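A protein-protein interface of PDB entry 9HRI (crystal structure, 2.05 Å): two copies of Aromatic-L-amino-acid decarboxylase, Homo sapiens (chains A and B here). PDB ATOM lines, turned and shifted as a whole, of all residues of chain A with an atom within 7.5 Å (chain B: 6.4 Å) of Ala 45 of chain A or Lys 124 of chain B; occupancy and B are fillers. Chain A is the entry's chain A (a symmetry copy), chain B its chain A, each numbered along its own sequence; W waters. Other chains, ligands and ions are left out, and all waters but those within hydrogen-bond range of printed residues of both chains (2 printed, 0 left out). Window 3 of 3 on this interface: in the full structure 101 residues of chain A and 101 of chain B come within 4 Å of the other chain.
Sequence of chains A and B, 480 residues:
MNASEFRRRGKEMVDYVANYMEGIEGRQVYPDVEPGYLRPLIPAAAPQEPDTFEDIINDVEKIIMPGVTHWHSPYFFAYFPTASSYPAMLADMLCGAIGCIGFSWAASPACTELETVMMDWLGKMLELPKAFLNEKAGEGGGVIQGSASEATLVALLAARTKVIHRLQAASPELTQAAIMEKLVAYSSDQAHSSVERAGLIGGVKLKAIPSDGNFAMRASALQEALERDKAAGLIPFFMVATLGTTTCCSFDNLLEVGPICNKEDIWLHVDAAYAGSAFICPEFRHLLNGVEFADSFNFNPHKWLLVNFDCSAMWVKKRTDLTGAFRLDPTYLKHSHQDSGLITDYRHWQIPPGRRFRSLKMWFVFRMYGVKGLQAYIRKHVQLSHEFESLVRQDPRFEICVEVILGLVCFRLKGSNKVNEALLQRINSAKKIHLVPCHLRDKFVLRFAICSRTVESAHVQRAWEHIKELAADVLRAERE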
ATOM      1  N   ARG A  39      -4.715  19.108  26.626  1.00  0.00           N
ATOM      2  CA  ARG A  39      -5.651  19.032  25.506  1.00  0.00           C
ATOM      3  C   ARG A  39      -5.378  20.041  24.395  1.00  0.00           C
ATOM      4  O   ARG A  39      -5.458  19.648  23.220  1.00  0.00           O
ATOM      5  CB  ARG A  39      -7.095  19.174  26.011  1.00  0.00           C
ATOM      6  CG  ARG A  39      -8.144  18.750  24.984  1.00  0.00           C
ATOM      7  CD  ARG A  39      -9.571  18.980  25.472  1.00  0.00           C
ATOM      8  NE  ARG A  39     -10.009  17.978  26.438  1.00  0.00           N
ATOM      9  CZ  ARG A  39     -10.468  16.774  26.125  1.00  0.00           C
ATOM     10  NH1 ARG A  39     -10.562  16.372  24.867  1.00  0.00           N
ATOM     11  NH2 ARG A  39     -10.844  15.951  27.100  1.00  0.00           N
ATOM     12  N   ILE A  42      -2.459  18.713  21.947  1.00  0.00           N
ATOM     13  CA  ILE A  42      -2.600  17.443  21.238  1.00  0.00           C
ATOM     14  C   ILE A  42      -3.752  17.590  20.249  1.00  0.00           C
ATOM     15  O   ILE A  42      -4.724  18.299  20.547  1.00  0.00           O
ATOM     16  CB  ILE A  42      -2.831  16.289  22.230  1.00  0.00           C
ATOM     17  CG1 ILE A  42      -1.573  16.060  23.065  1.00  0.00           C
ATOM     18  CG2 ILE A  42      -3.248  15.001  21.525  1.00  0.00           C
ATOM     19  CD1 ILE A  42      -1.686  14.908  24.040  1.00  0.00           C
ATOM     20  N   PRO A  43      -3.683  16.980  19.064  1.00  0.00           N
ATOM     21  CA  PRO A  43      -4.827  17.027  18.146  1.00  0.00           C
ATOM     22  C   PRO A  43      -6.086  16.454  18.778  1.00  0.00           C
ATOM     23  O   PRO A  43      -6.043  15.678  19.735  1.00  0.00           O
ATOM     24  CB  PRO A  43      -4.356  16.177  16.960  1.00  0.00           C
ATOM     25  CG  PRO A  43      -2.868  16.409  16.962  1.00  0.00           C
ATOM     26  CD  PRO A  43      -2.524  16.322  18.432  1.00  0.00           C
ATOM     27  N   ALA A  44      -7.227  16.857  18.221  1.00  0.00           N
ATOM     28  CA  ALA A  44      -8.520  16.448  18.752  1.00  0.00           C
ATOM     29  C   ALA A  44      -8.915  15.032  18.351  1.00  0.00           C
ATOM     30  O   ALA A  44      -9.847  14.478  18.944  1.00  0.00           O
ATOM     31  CB  ALA A  44      -9.603  17.431  18.301  1.00  0.00           C
ATOM     32  N   ALA A  45      -8.237  14.434  17.373  1.00  0.00           N
ATOM     33  CA  ALA A  45      -8.560  13.088  16.923  1.00  0.00           C
ATOM     34  C   ALA A  45      -7.276  12.318  16.650  1.00  0.00           C
ATOM     35  O   ALA A  45      -6.213  12.900  16.418  1.00  0.00           O
ATOM     36  CB  ALA A  45      -9.439  13.108  15.667  1.00  0.00           C
ATOM     37  N   ALA A  46      -7.391  10.992  16.686  1.00  0.00           N
ATOM     38  CA  ALA A  46      -6.256  10.140  16.372  1.00  0.00           C
ATOM     39  C   ALA A  46      -5.853  10.328  14.909  1.00  0.00           C
ATOM     40  O   ALA A  46      -6.696  10.635  14.061  1.00  0.00           O
ATOM     41  CB  ALA A  46      -6.594   8.674  16.639  1.00  0.00           C
ATOM     42  N   PRO A  47      -4.572  10.160  14.587  1.00  0.00           N
ATOM     43  CA  PRO A  47      -4.147  10.283  13.190  1.00  0.00           C
ATOM     44  C   PRO A  47      -4.626   9.101  12.364  1.00  0.00           C
ATOM     45  O   PRO A  47      -4.672   7.963  12.836  1.00  0.00           O
ATOM     46  CB  PRO A  47      -2.618  10.309  13.294  1.00  0.00           C
ATOM     47  CG  PRO A  47      -2.350   9.461  14.498  1.00  0.00           C
ATOM     48  CD  PRO A  47      -3.427   9.887  15.473  1.00  0.00           C
ATOM     49  N   GLN A  48      -4.995   9.382  11.114  1.00  0.00           N
ATOM     50  CA  GLN A  48      -5.392   8.309  10.210  1.00  0.00           C
ATOM     51  C   GLN A  48      -4.176   7.545   9.696  1.00  0.00           C
ATOM     52  O   GLN A  48      -4.179   6.308   9.676  1.00  0.00           O
ATOM     53  CB  GLN A  48      -6.208   8.879   9.049  1.00  0.00           C
ATOM     54  CG  GLN A  48      -7.585   9.392   9.464  1.00  0.00           C
ATOM     55  CD  GLN A  48      -8.594   8.279   9.689  1.00  0.00           C
ATOM     56  OE1 GLN A  48      -8.671   7.327   8.914  1.00  0.00           O
ATOM     57  NE2 GLN A  48      -9.369   8.394  10.762  1.00  0.00           N
ATOM     58  N   MET B 119      -9.154   8.789  25.783  1.00  0.00           N
ATOM     59  CA  MET B 119     -10.504   8.234  25.806  1.00  0.00           C
ATOM     60  C   MET B 119     -11.432   8.987  24.862  1.00  0.00           C
ATOM     61  O   MET B 119     -12.399   8.407  24.357  1.00  0.00           O
ATOM     62  CB  MET B 119     -11.060   8.244  27.233  1.00  0.00           C
ATOM     63  CG  MET B 119     -10.417   7.208  28.145  1.00  0.00           C
ATOM     64  SD  MET B 119     -10.634   5.511  27.568  1.00  0.00           S
ATOM     65  CE  MET B 119     -12.326   5.200  28.071  1.00  0.00           C
ATOM     66  N   ASP B 120     -11.156  10.270  24.610  1.00  0.00           N
ATOM     67  CA  ASP B 120     -11.915  11.002  23.601  1.00  0.00           C
ATOM     68  C   ASP B 120     -11.514  10.577  22.194  1.00  0.00           C
ATOM     69  O   ASP B 120     -12.373  10.423  21.318  1.00  0.00           O
ATOM     70  CB  ASP B 120     -11.721  12.509  23.786  1.00  0.00           C
ATOM     71  CG  ASP B 120     -12.588  13.076  24.895  1.00  0.00           C
ATOM     72  OD1 ASP B 120     -13.516  12.372  25.343  1.00  0.00           O
ATOM     73  OD2 ASP B 120     -12.341  14.221  25.324  1.00  0.00           O
ATOM     74  N   TRP B 121     -10.210  10.395  21.958  1.00  0.00           N
ATOM     75  CA  TRP B 121      -9.741   9.826  20.697  1.00  0.00           C
ATOM     76  C   TRP B 121     -10.466   8.523  20.384  1.00  0.00           C
ATOM     77  O   TRP B 121     -11.046   8.356  19.304  1.00  0.00           O
ATOM     78  CB  TRP B 121      -8.232   9.577  20.765  1.00  0.00           C
ATOM     79  CG  TRP B 121      -7.355  10.736  20.382  1.00  0.00           C
ATOM     80  CD1 TRP B 121      -7.680  12.060  20.394  1.00  0.00           C
ATOM     81  CD2 TRP B 121      -5.998  10.658  19.927  1.00  0.00           C
ATOM     82  NE1 TRP B 121      -6.606  12.814  19.977  1.00  0.00           N
ATOM     83  CE2 TRP B 121      -5.562  11.976  19.684  1.00  0.00           C
ATOM     84  CE3 TRP B 121      -5.110   9.601  19.706  1.00  0.00           C
ATOM     85  CZ2 TRP B 121      -4.273  12.263  19.229  1.00  0.00           C
ATOM     86  CZ3 TRP B 121      -3.834   9.887  19.250  1.00  0.00           C
ATOM     87  CH2 TRP B 121      -3.428  11.208  19.019  1.00  0.00           C
ATOM     88  N   LEU B 122     -10.443   7.588  21.336  1.00  0.00           N
ATOM     89  CA  LEU B 122     -11.041   6.273  21.128  1.00  0.00           C
ATOM     90  C   LEU B 122     -12.557   6.362  21.018  1.00  0.00           C
ATOM     91  O   LEU B 122     -13.168   5.664  20.200  1.00  0.00           O
ATOM     92  CB  LEU B 122     -10.637   5.345  22.273  1.00  0.00           C
ATOM     93  CG  LEU B 122     -10.944   3.852  22.145  1.00  0.00           C
ATOM     94  CD1 LEU B 122     -10.502   3.323  20.788  1.00  0.00           C
ATOM     95  CD2 LEU B 122     -10.272   3.087  23.277  1.00  0.00           C
ATOM     96  N   GLY B 123     -13.183   7.208  21.838  1.00  0.00           N
ATOM     97  CA  GLY B 123     -14.625   7.372  21.749  1.00  0.00           C
ATOM     98  C   GLY B 123     -15.062   7.882  20.390  1.00  0.00           C
ATOM     99  O   GLY B 123     -16.104   7.475  19.867  1.00  0.00           O
ATOM    100  N   LYS B 124     -14.267   8.771  19.793  1.00  0.00           N
ATOM    101  CA  LYS B 124     -14.593   9.267  18.464  1.00  0.00           C
ATOM    102  C   LYS B 124     -14.300   8.223  17.397  1.00  0.00           C
ATOM    103  O   LYS B 124     -15.020   8.143  16.396  1.00  0.00           O
ATOM    104  CB  LYS B 124     -13.825  10.559  18.186  1.00  0.00           C
ATOM    105  CG  LYS B 124     -14.353  11.750  18.978  1.00  0.00           C
ATOM    106  CD  LYS B 124     -13.270  12.783  19.251  1.00  0.00           C
ATOM    107  CE  LYS B 124     -12.678  13.311  17.961  1.00  0.00           C
ATOM    108  NZ  LYS B 124     -13.650  14.158  17.215  1.00  0.00           N
ATOM    109  N   MET B 125     -13.254   7.413  17.593  1.00  0.00           N
ATOM    110  CA  MET B 125     -12.983   6.323  16.664  1.00  0.00           C
ATOM    111  C   MET B 125     -14.135   5.330  16.630  1.00  0.00           C
ATOM    112  O   MET B 125     -14.437   4.759  15.576  1.00  0.00           O
ATOM    113  CB  MET B 125     -11.689   5.605  17.047  1.00  0.00           C
ATOM    114  CG  MET B 125     -10.425   6.327  16.623  1.00  0.00           C
ATOM    115  SD  MET B 125      -9.001   5.836  17.614  1.00  0.00           S
ATOM    116  CE  MET B 125      -9.026   4.065  17.338  1.00  0.00           C
ATOM    117  N   LEU B 126     -14.784   5.109  17.770  1.00  0.00           N
ATOM    118  CA  LEU B 126     -15.929   4.213  17.830  1.00  0.00           C
ATOM    119  C   LEU B 126     -17.229   4.904  17.452  1.00  0.00           C
ATOM    120  O   LEU B 126     -18.280   4.254  17.469  1.00  0.00           O
ATOM    121  CB  LEU B 126     -16.068   3.622  19.231  1.00  0.00           C
ATOM    122  CG  LEU B 126     -15.406   2.268  19.490  1.00  0.00           C
ATOM    123  CD1 LEU B 126     -13.899   2.447  19.574  1.00  0.00           C
ATOM    124  CD2 LEU B 126     -15.966   1.617  20.747  1.00  0.00           C
ATOM    125  N   GLU B 127     -17.176   6.196  17.116  1.00  0.00           N
ATOM    126  CA  GLU B 127     -18.369   6.997  16.834  1.00  0.00           C
ATOM    127  C   GLU B 127     -19.387   6.867  17.964  1.00  0.00           C
ATOM    128  O   GLU B 127     -20.587   6.691  17.739  1.00  0.00           O
ATOM    129  CB  GLU B 127     -18.982   6.623  15.483  1.00  0.00           C
ATOM    130  CG  GLU B 127     -18.017   6.809  14.319  1.00  0.00           C
ATOM    131  CD  GLU B 127     -18.707   6.767  12.970  1.00  0.00           C
ATOM    132  OE1 GLU B 127     -19.057   7.849  12.451  1.00  0.00           O
ATOM    133  OE2 GLU B 127     -18.889   5.658  12.422  1.00  0.00           O
ATOM    134  N   LEU B 128     -18.893   6.935  19.197  1.00  0.00           N
ATOM    135  CA  LEU B 128     -19.756   6.854  20.362  1.00  0.00           C
ATOM    136  C   LEU B 128     -20.654   8.088  20.442  1.00  0.00           C
ATOM    137  O   LEU B 128     -20.277   9.169  19.983  1.00  0.00           O
ATOM    138  CB  LEU B 128     -18.919   6.745  21.636  1.00  0.00           C
ATOM    139  CG  LEU B 128     -18.267   5.402  21.982  1.00  0.00           C
ATOM    140  CD1 LEU B 128     -17.652   5.468  23.371  1.00  0.00           C
ATOM    141  CD2 LEU B 128     -19.256   4.246  21.880  1.00  0.00           C
ATOM    142  N   LEU B 133     -18.401  11.385  25.902  1.00  0.00           N
ATOM    143  CA  LEU B 133     -17.080  11.966  25.700  1.00  0.00           C
ATOM    144  C   LEU B 133     -16.734  12.988  26.782  1.00  0.00           C
ATOM    145  O   LEU B 133     -17.578  13.792  27.191  1.00  0.00           O
ATOM    146  CB  LEU B 133     -17.002  12.622  24.320  1.00  0.00           C
ATOM    147  CG  LEU B 133     -17.332  11.721  23.126  1.00  0.00           C
ATOM    148  CD1 LEU B 133     -16.902  12.367  21.817  1.00  0.00           C
ATOM    149  CD2 LEU B 133     -16.682  10.351  23.279  1.00  0.00           C
ATOM    150  N   GLU B 135     -15.103  15.391  26.102  1.00  0.00           N
ATOM    151  CA  GLU B 135     -14.755  16.545  25.291  1.00  0.00           C
ATOM    152  C   GLU B 135     -15.792  17.660  25.409  1.00  0.00           C
ATOM    153  O   GLU B 135     -16.975  17.429  25.683  1.00  0.00           O
ATOM    154  CB  GLU B 135     -14.607  16.098  23.837  1.00  0.00           C
ATOM    155  CG  GLU B 135     -14.076  17.115  22.853  1.00  0.00           C
ATOM    156  CD  GLU B 135     -14.303  16.657  21.425  1.00  0.00           C
ATOM    157  OE1 GLU B 135     -13.350  16.701  20.623  1.00  0.00           O
ATOM    158  OE2 GLU B 135     -15.435  16.234  21.110  1.00  0.00           O
ATOM    159  N   TRP B 315     -16.519   4.032  29.339  1.00  0.00           N
ATOM    160  CA  TRP B 315     -17.190   5.322  29.275  1.00  0.00           C
ATOM    161  C   TRP B 315     -18.461   5.277  30.112  1.00  0.00           C
ATOM    162  O   TRP B 315     -19.172   4.267  30.127  1.00  0.00           O
ATOM    163  CB  TRP B 315     -17.544   5.701  27.832  1.00  0.00           C
ATOM    164  CG  TRP B 315     -16.362   5.995  26.953  1.00  0.00           C
ATOM    165  CD1 TRP B 315     -15.852   7.225  26.653  1.00  0.00           C
ATOM    166  CD2 TRP B 315     -15.569   5.045  26.232  1.00  0.00           C
ATOM    167  NE1 TRP B 315     -14.779   7.099  25.805  1.00  0.00           N
ATOM    168  CE2 TRP B 315     -14.586   5.770  25.529  1.00  0.00           C
ATOM    169  CE3 TRP B 315     -15.591   3.651  26.117  1.00  0.00           C
ATOM    170  CZ2 TRP B 315     -13.631   5.149  24.727  1.00  0.00           C
ATOM    171  CZ3 TRP B 315     -14.641   3.037  25.316  1.00  0.00           C
ATOM    172  CH2 TRP B 315     -13.676   3.786  24.632  1.00  0.00           C
HETATM  173  O   HOH W   1     -10.971  15.131  21.397  1.00  0.00           O
HETATM  174  O   HOH W   2     -10.067   9.922  17.120  1.00  0.00           O
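The guanidinium group (NH1) of Arg 39 of chain A lies within salt-bridge range of the side-chain carboxylate (OD2) of Asp 120 of chain B (2.8 Å). NE1 of Trp 121 of chain B sits at hydrogen-bond distance from O of Pro 43 of chain A (2.9 Å). The backbone NH (N) of Ala 45 of chain A sits close to the indole nitrogen (NE1) of Trp 121 of chain B.
The backbone NH of Glu 135 of chain B lies within hydrogen-bond range of the side-chain carboxylate of Asp 120 of chain B, at 3.1 Å.
CG2 of Ile 42 of chain A touches CZ2 of Trp 121 of chain B (3.7 Å). O of Ala 44 of chain A touches CD1 of Trp 121 of chain B (3.6 Å). O of Ala 44 of chain A touches CE of Lys 124 of chain B (3.2 Å). Lys 124 of chain B touches Ala 45 of chain A. CB of Ala 46 of chain A touches CE3 of Trp 121 of chain B, at 3.5 Å. Ala 46 of chain A touches Met 125 of chain B. CD of Pro 47 of chain A touches CH2 of Trp 121 of chain B, at 3.8 Å.
Printed residues of chain B within 4 Å of Arg 39 of chain A: Asp 120 (2.8 Å). Printed residues of chain B within 4 Å of Ile 42 of chain A: Trp 121. Of the printed residues of chain B, Ala 44 of chain A touches Trp 121 and Lys 124. Leu 122 of chain B touches none of the printed residues of chain A. No residue of chain A comes within 4 Å of Gly 123 of chain B. Lys 124 of chain B touches just these residues of chain A: Ala 44 (3.2 Å) and Ala 45 (3.97 Å). The nearest printed residue of chain B that does not touch Ala 45 of chain A is Asp 120 of chain B (6.4 Å). The nearest residue of chain A that does not touch Lys 124 of chain B is Ala 46 of chain A (5.9 Å).
Of the 13 printed residues of chain B, 4 touch a printed residue of chain A. Hydrophobic or aromatic side chains of chain A within 4 Å of the printed part of chain B: Ile 42, Ala 45, Ala 46 and Pro 47. Among the printed residues, Asp or Glu carboxylates within 4 Å of a Lys or Arg side-chain nitrogen of the other chain: Arg 39 of chain A with Asp 120 of chain B (2.8 Å).
No position is printed for both chains.
Water W1 lies within hydrogen-bond range of O of Ala 44 of chain A and OE1 of Glu 135 of chain B. Water W2 lies within hydrogen-bond range of the backbone carbonyl oxygen of Trp 121 of chain B and the backbone NH of Ala 46 of chain A.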
